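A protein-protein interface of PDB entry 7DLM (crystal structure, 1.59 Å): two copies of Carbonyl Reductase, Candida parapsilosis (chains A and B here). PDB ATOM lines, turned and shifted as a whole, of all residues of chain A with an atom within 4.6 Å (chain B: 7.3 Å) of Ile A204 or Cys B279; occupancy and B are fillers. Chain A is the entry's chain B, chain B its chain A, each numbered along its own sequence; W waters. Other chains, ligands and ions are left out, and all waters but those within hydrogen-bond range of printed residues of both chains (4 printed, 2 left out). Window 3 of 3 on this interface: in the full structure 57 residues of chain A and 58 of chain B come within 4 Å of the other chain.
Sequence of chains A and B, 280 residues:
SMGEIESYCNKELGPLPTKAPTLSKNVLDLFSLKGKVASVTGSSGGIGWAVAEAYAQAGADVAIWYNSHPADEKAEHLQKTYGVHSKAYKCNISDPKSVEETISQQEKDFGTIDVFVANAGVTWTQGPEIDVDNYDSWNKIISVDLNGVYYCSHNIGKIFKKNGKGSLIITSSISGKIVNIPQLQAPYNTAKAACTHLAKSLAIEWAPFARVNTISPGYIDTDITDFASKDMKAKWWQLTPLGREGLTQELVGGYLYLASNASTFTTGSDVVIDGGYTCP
O of Leu B239 lies within hydrogen-bond range of SG of Cys A9, 3.6 Å away. O of Gly A268 lies within hydrogen-bond range of SG of Cys B279, at 3.1 Å.
The side-chain amino group of Lys A200 sits at hydrogen-bond distance from the backbone carbonyl oxygen of Gly A268, 2.9 Å away. The side-chain amide nitrogen of Asn A10 sits at hydrogen-bond distance from the backbone carbonyl oxygen of Ile A204, 3.1 Å away.
SG of Cys A9 touches C of Thr B240 (3.9 Å). N of Pro B241 touches SG of Cys A9 (3.8 Å). Lys A200 touches Cys B279. CG1 of Ile A204 touches CG of Pro B241 (3.6 Å). Ile A204 touches Cys B279. Ala A207 touches Pro B241 (CB to O, 3.1 Å).
Of the printed residues of chain B, Lys A200 touches Cys B279 (3.7 Å). Ser A201 touches none of the printed residues of chain B. No residue of chain B comes within 4 Å of Ala A203. Of chain B, only Pro B241 and Cys B279 come within 4 Å of Ile A204. Of the printed residues of chain A, Leu B239 touches Cys A9. Printed residues of chain A within 4 Å of Thr B240: Cys A9 (3.9 Å). Cys B279 touches just these residues of chain A: Lys A200, Ile A204 and Gly A268. The nearest residue of chain B that does not touch Ile A204 is Pro B280 (4.5 Å).
Of the 12 printed residues of chain B, 4 touch a printed residue of chain A. Hydrophobic or aromatic side chains of chain A that line the printed part of chain B: Ile A204 and Ala A207. Along chain A the printed residues that touch a printed residue of chain B span positions 9 to 268. Among the printed residues, 8 pairs touch across the chains.
No position is printed for both chains.
Water W1 bridges the side-chain carboxylate (OD1) of Asp B274 (2.8 Å) and the backbone carbonyl oxygen (O) of Gly A268 (3.3 Å). Water W4 bridges the backbone carbonyl oxygen (O) of Leu B242 (2.8 Å) and the backbone carbonyl oxygen (O) of Ala A207 (3.0 Å). Water W2 bridges the backbone carbonyl oxygen (O) of Pro B241 (2.9 Å) and the backbone carbonyl oxygen (O) of Ile A204 (2.9 Å). Water W3 lies within hydrogen-bond range of NZ of Lys A200 and O of Thr B278.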
ATOM      1  N   CYS A   9       8.065 -23.391 -26.167  1.00  0.00           N
ATOM      2  CA  CYS A   9       9.228 -24.159 -26.601  1.00  0.00           C
ATOM      3  C   CYS A   9       9.193 -25.614 -26.130  1.00  0.00           C
ATOM      4  O   CYS A   9       9.422 -26.519 -26.934  1.00  0.00           O
ATOM      5  CB  CYS A   9      10.526 -23.485 -26.105  1.00  0.00           C
ATOM      6  SG  CYS A   9      10.876 -21.847 -26.753  1.00  0.00           S
ATOM      7  N   ASN A  10       8.936 -25.864 -24.844  1.00  0.00           N
ATOM      8  CA  ASN A  10       9.111 -27.208 -24.280  1.00  0.00           C
ATOM      9  C   ASN A  10       8.346 -27.270 -22.964  1.00  0.00           C
ATOM     10  O   ASN A  10       8.767 -26.637 -21.988  1.00  0.00           O
ATOM     11  CB  ASN A  10      10.610 -27.501 -24.081  1.00  0.00           C
ATOM     12  CG  ASN A  10      10.857 -28.923 -23.692  1.00  0.00           C
ATOM     13  OD1 ASN A  10       9.963 -29.603 -23.196  1.00  0.00           O
ATOM     14  ND2 ASN A  10      12.097 -29.383 -23.867  1.00  0.00           N
ATOM     15  N   LYS A 200      21.533 -26.576 -32.049  1.00  0.00           N
ATOM     16  CA  LYS A 200      20.458 -25.637 -31.737  1.00  0.00           C
ATOM     17  C   LYS A 200      19.154 -26.374 -31.448  1.00  0.00           C
ATOM     18  O   LYS A 200      18.427 -26.015 -30.511  1.00  0.00           O
ATOM     19  CB  LYS A 200      20.285 -24.630 -32.883  1.00  0.00           C
ATOM     20  CG  LYS A 200      21.426 -23.614 -32.982  1.00  0.00           C
ATOM     21  CD  LYS A 200      21.307 -22.769 -34.242  1.00  0.00           C
ATOM     22  CE  LYS A 200      22.508 -21.859 -34.415  1.00  0.00           C
ATOM     23  NZ  LYS A 200      22.463 -20.786 -33.362  1.00  0.00           N
ATOM     24  N   SER A 201      18.850 -27.416 -32.230  1.00  0.00           N
ATOM     25  CA  SER A 201      17.608 -28.166 -32.035  1.00  0.00           C
ATOM     26  C   SER A 201      17.582 -28.873 -30.683  1.00  0.00           C
ATOM     27  O   SER A 201      16.556 -28.857 -29.982  1.00  0.00           O
ATOM     28  CB  SER A 201      17.435 -29.180 -33.167  1.00  0.00           C
ATOM     29  OG  SER A 201      17.266 -28.532 -34.420  1.00  0.00           O
ATOM     30  N   LEU A 202      18.697 -29.510 -30.307  1.00  0.00           N
ATOM     31  CA  LEU A 202      18.796 -30.153 -28.996  1.00  0.00           C
ATOM     32  C   LEU A 202      18.765 -29.136 -27.853  1.00  0.00           C
ATOM     33  O   LEU A 202      18.281 -29.451 -26.759  1.00  0.00           O
ATOM     34  CB  LEU A 202      20.070 -31.004 -28.918  1.00  0.00           C
ATOM     35  CG  LEU A 202      20.100 -32.203 -29.876  1.00  0.00           C
ATOM     36  CD1 LEU A 202      21.420 -32.966 -29.691  1.00  0.00           C
ATOM     37  CD2 LEU A 202      18.874 -33.112 -29.644  1.00  0.00           C
ATOM     38  N   ALA A 203      19.236 -27.904 -28.081  1.00  0.00           N
ATOM     39  CA  ALA A 203      19.157 -26.886 -27.031  1.00  0.00           C
ATOM     40  C   ALA A 203      17.714 -26.664 -26.576  1.00  0.00           C
ATOM     41  O   ALA A 203      17.447 -26.525 -25.378  1.00  0.00           O
ATOM     42  CB  ALA A 203      19.769 -25.570 -27.518  1.00  0.00           C
ATOM     43  N   ILE A 204      16.769 -26.618 -27.511  1.00  0.00           N
ATOM     44  CA  ILE A 204      15.354 -26.574 -27.121  1.00  0.00           C
ATOM     45  C   ILE A 204      14.893 -27.856 -26.438  1.00  0.00           C
ATOM     46  O   ILE A 204      14.232 -27.791 -25.394  1.00  0.00           O
ATOM     47  CB  ILE A 204      14.464 -26.167 -28.312  1.00  0.00           C
ATOM     48  CG1 ILE A 204      14.778 -24.699 -28.671  1.00  0.00           C
ATOM     49  CG2 ILE A 204      12.977 -26.549 -28.044  1.00  0.00           C
ATOM     50  CD1 ILE A 204      15.886 -24.395 -29.608  1.00  0.00           C
ATOM     51  N   GLU A 205      15.221 -29.023 -26.996  1.00  0.00           N
ATOM     52  CA  GLU A 205      14.658 -30.260 -26.458  1.00  0.00           C
ATOM     53  C   GLU A 205      15.201 -30.567 -25.066  1.00  0.00           C
ATOM     54  O   GLU A 205      14.471 -31.130 -24.238  1.00  0.00           O
ATOM     55  CB  GLU A 205      14.934 -31.432 -27.413  1.00  0.00           C
ATOM     56  CG  GLU A 205      14.469 -31.145 -28.856  1.00  0.00           C
ATOM     57  CD  GLU A 205      14.215 -32.394 -29.699  1.00  0.00           C
ATOM     58  OE1 GLU A 205      13.965 -32.245 -30.915  1.00  0.00           O
ATOM     59  OE2 GLU A 205      14.268 -33.526 -29.173  1.00  0.00           O
ATOM     60  N   TRP A 206      16.450 -30.180 -24.781  1.00  0.00           N
ATOM     61  CA  TRP A 206      17.110 -30.542 -23.525  1.00  0.00           C
ATOM     62  C   TRP A 206      17.091 -29.430 -22.491  1.00  0.00           C
ATOM     63  O   TRP A 206      17.647 -29.604 -21.401  1.00  0.00           O
ATOM     64  CB  TRP A 206      18.571 -30.925 -23.770  1.00  0.00           C
ATOM     65  CG  TRP A 206      18.848 -32.148 -24.580  1.00  0.00           C
ATOM     66  CD1 TRP A 206      17.963 -32.924 -25.277  1.00  0.00           C
ATOM     67  CD2 TRP A 206      20.134 -32.734 -24.770  1.00  0.00           C
ATOM     68  NE1 TRP A 206      18.632 -33.952 -25.902  1.00  0.00           N
ATOM     69  CE2 TRP A 206      19.967 -33.857 -25.600  1.00  0.00           C
ATOM     70  CE3 TRP A 206      21.416 -32.408 -24.319  1.00  0.00           C
ATOM     71  CZ2 TRP A 206      21.037 -34.650 -26.002  1.00  0.00           C
ATOM     72  CZ3 TRP A 206      22.477 -33.197 -24.708  1.00  0.00           C
ATOM     73  CH2 TRP A 206      22.285 -34.309 -25.532  1.00  0.00           C
ATOM     74  N   ALA A 207      16.465 -28.292 -22.800  1.00  0.00           N
ATOM     75  CA  ALA A 207      16.488 -27.110 -21.945  1.00  0.00           C
ATOM     76  C   ALA A 207      16.140 -27.353 -20.473  1.00  0.00           C
ATOM     77  O   ALA A 207      16.702 -26.671 -19.605  1.00  0.00           O
ATOM     78  CB  ALA A 207      15.559 -26.057 -22.545  1.00  0.00           C
ATOM     79  N   GLY A 268      22.221 -23.052 -27.307  1.00  0.00           N
ATOM     80  CA  GLY A 268      21.892 -22.885 -28.710  1.00  0.00           C
ATOM     81  C   GLY A 268      22.807 -21.946 -29.462  1.00  0.00           C
ATOM     82  O   GLY A 268      22.450 -21.496 -30.557  1.00  0.00           O
ATOM     83  N   ILE B 178      17.240 -10.550 -34.521  1.00  0.00           N
ATOM     84  CA  ILE B 178      15.825 -10.854 -34.630  1.00  0.00           C
ATOM     85  C   ILE B 178      15.019  -9.584 -34.397  1.00  0.00           C
ATOM     86  O   ILE B 178      15.543  -8.558 -33.967  1.00  0.00           O
ATOM     87  CB  ILE B 178      15.366 -11.881 -33.600  1.00  0.00           C
ATOM     88  CG1 ILE B 178      15.608 -11.134 -32.272  1.00  0.00           C
ATOM     89  CG2 ILE B 178      16.072 -13.233 -33.902  1.00  0.00           C
ATOM     90  CD1 ILE B 178      15.083 -11.622 -31.084  1.00  0.00           C
ATOM     91  N   LEU B 239       8.811 -17.845 -25.123  1.00  0.00           N
ATOM     92  CA  LEU B 239       9.583 -17.966 -26.351  1.00  0.00           C
ATOM     93  C   LEU B 239      11.073 -18.207 -26.101  1.00  0.00           C
ATOM     94  O   LEU B 239      11.824 -18.377 -27.063  1.00  0.00           O
ATOM     95  CB  LEU B 239       9.381 -16.699 -27.206  1.00  0.00           C
ATOM     96  CG  LEU B 239       7.941 -16.451 -27.692  1.00  0.00           C
ATOM     97  CD1 LEU B 239       7.854 -15.218 -28.611  1.00  0.00           C
ATOM     98  CD2 LEU B 239       7.412 -17.665 -28.398  1.00  0.00           C
ATOM     99  N   THR B 240      11.523 -18.229 -24.838  1.00  0.00           N
ATOM    100  CA  THR B 240      12.931 -18.458 -24.507  1.00  0.00           C
ATOM    101  C   THR B 240      13.158 -19.927 -24.173  1.00  0.00           C
ATOM    102  O   THR B 240      12.564 -20.421 -23.198  1.00  0.00           O
ATOM    103  CB  THR B 240      13.342 -17.597 -23.312  1.00  0.00           C
ATOM    104  OG1 THR B 240      13.073 -16.211 -23.576  1.00  0.00           O
ATOM    105  CG2 THR B 240      14.860 -17.769 -23.044  1.00  0.00           C
ATOM    106  N   PRO B 241      13.993 -20.665 -24.908  1.00  0.00           N
ATOM    107  CA  PRO B 241      14.193 -22.097 -24.587  1.00  0.00           C
ATOM    108  C   PRO B 241      14.532 -22.406 -23.129  1.00  0.00           C
ATOM    109  O   PRO B 241      14.040 -23.411 -22.604  1.00  0.00           O
ATOM    110  CB  PRO B 241      15.328 -22.490 -25.537  1.00  0.00           C
ATOM    111  CG  PRO B 241      15.004 -21.678 -26.753  1.00  0.00           C
ATOM    112  CD  PRO B 241      14.585 -20.322 -26.215  1.00  0.00           C
ATOM    113  N   LEU B 242      15.324 -21.574 -22.448  1.00  0.00           N
ATOM    114  CA  LEU B 242      15.604 -21.868 -21.036  1.00  0.00           C
ATOM    115  C   LEU B 242      14.467 -21.464 -20.109  1.00  0.00           C
ATOM    116  O   LEU B 242      14.436 -21.927 -18.956  1.00  0.00           O
ATOM    117  CB  LEU B 242      16.892 -21.187 -20.566  1.00  0.00           C
ATOM    118  CG  LEU B 242      18.197 -21.713 -21.161  1.00  0.00           C
ATOM    119  CD1 LEU B 242      19.405 -21.081 -20.424  1.00  0.00           C
ATOM    120  CD2 LEU B 242      18.235 -23.242 -21.099  1.00  0.00           C
ATOM    121  N   ASP B 274      21.610 -15.663 -24.576  1.00  0.00           N
ATOM    122  CA  ASP B 274      20.192 -15.319 -24.704  1.00  0.00           C
ATOM    123  C   ASP B 274      19.250 -16.440 -24.268  1.00  0.00           C
ATOM    124  O   ASP B 274      18.058 -16.393 -24.602  1.00  0.00           O
ATOM    125  CB  ASP B 274      19.861 -14.901 -26.163  1.00  0.00           C
ATOM    126  CG  ASP B 274      19.916 -16.070 -27.170  1.00  0.00           C
ATOM    127  OD1 ASP B 274      20.416 -17.170 -26.849  1.00  0.00           O
ATOM    128  OD2 ASP B 274      19.466 -15.872 -28.329  1.00  0.00           O
ATOM    129  N   GLY B 275      19.742 -17.448 -23.552  1.00  0.00           N
ATOM    130  CA  GLY B 275      18.889 -18.564 -23.166  1.00  0.00           C
ATOM    131  C   GLY B 275      18.273 -19.301 -24.327  1.00  0.00           C
ATOM    132  O   GLY B 275      17.245 -19.971 -24.151  1.00  0.00           O
ATOM    133  N   GLY B 276      18.857 -19.179 -25.527  1.00  0.00           N
ATOM    134  CA  GLY B 276      18.344 -19.836 -26.720  1.00  0.00           C
ATOM    135  C   GLY B 276      17.354 -19.032 -27.544  1.00  0.00           C
ATOM    136  O   GLY B 276      16.824 -19.574 -28.529  1.00  0.00           O
ATOM    137  N   TYR B 277      17.084 -17.770 -27.178  1.00  0.00           N
ATOM    138  CA  TYR B 277      15.970 -17.014 -27.775  1.00  0.00           C
ATOM    139  C   TYR B 277      16.029 -16.962 -29.302  1.00  0.00           C
ATOM    140  O   TYR B 277      14.989 -17.033 -29.975  1.00  0.00           O
ATOM    141  CB  TYR B 277      15.912 -15.577 -27.222  1.00  0.00           C
ATOM    142  CG  TYR B 277      14.626 -14.887 -27.646  1.00  0.00           C
ATOM    143  CD1 TYR B 277      14.547 -14.230 -28.871  1.00  0.00           C
ATOM    144  CD2 TYR B 277      13.473 -14.952 -26.864  1.00  0.00           C
ATOM    145  CE1 TYR B 277      13.373 -13.656 -29.282  1.00  0.00           C
ATOM    146  CE2 TYR B 277      12.293 -14.358 -27.282  1.00  0.00           C
ATOM    147  CZ  TYR B 277      12.255 -13.721 -28.496  1.00  0.00           C
ATOM    148  OH  TYR B 277      11.106 -13.122 -28.965  1.00  0.00           O
ATOM    149  N   THR B 278      17.219 -16.780 -29.867  1.00  0.00           N
ATOM    150  CA  THR B 278      17.352 -16.623 -31.307  1.00  0.00           C
ATOM    151  C   THR B 278      17.237 -17.940 -32.077  1.00  0.00           C
ATOM    152  O   THR B 278      17.282 -17.915 -33.315  1.00  0.00           O
ATOM    153  CB  THR B 278      18.689 -15.933 -31.640  1.00  0.00           C
ATOM    154  OG1 THR B 278      19.763 -16.594 -30.958  1.00  0.00           O
ATOM    155  CG2 THR B 278      18.662 -14.477 -31.207  1.00  0.00           C
ATOM    156  N   CYS B 279      17.088 -19.080 -31.397  1.00  0.00           N
ATOM    157  CA  CYS B 279      17.026 -20.380 -32.082  1.00  0.00           C
ATOM    158  C   CYS B 279      15.652 -20.744 -32.655  1.00  0.00           C
ATOM    159  O   CYS B 279      15.591 -21.162 -33.817  1.00  0.00           O
ATOM    160  CB  CYS B 279      17.525 -21.499 -31.146  1.00  0.00           C
ATOM    161  SG  CYS B 279      19.326 -21.446 -30.884  1.00  0.00           S
ATOM    162  N   PRO B 280      14.529 -20.625 -31.907  1.00  0.00           N
ATOM    163  CA  PRO B 280      13.267 -21.186 -32.440  1.00  0.00           C
ATOM    164  C   PRO B 280      12.802 -20.772 -33.855  1.00  0.00           C
ATOM    165  O   PRO B 280      12.168 -19.747 -34.189  1.00  0.00           O
ATOM    166  CB  PRO B 280      12.242 -20.772 -31.377  1.00  0.00           C
ATOM    167  CG  PRO B 280      13.067 -20.816 -30.092  1.00  0.00           C
ATOM    168  CD  PRO B 280      14.390 -20.210 -30.496  1.00  0.00           C
HETATM  169  O   HOH W   1      21.466 -18.896 -28.826  1.00  0.00           O
HETATM  170  O   HOH W   2      13.071 -25.171 -24.702  1.00  0.00           O
HETATM  171  O   HOH W   3      20.266 -19.048 -34.478  1.00  0.00           O
HETATM  172  O   HOH W   4      15.995 -24.140 -18.065  1.00  0.00           O
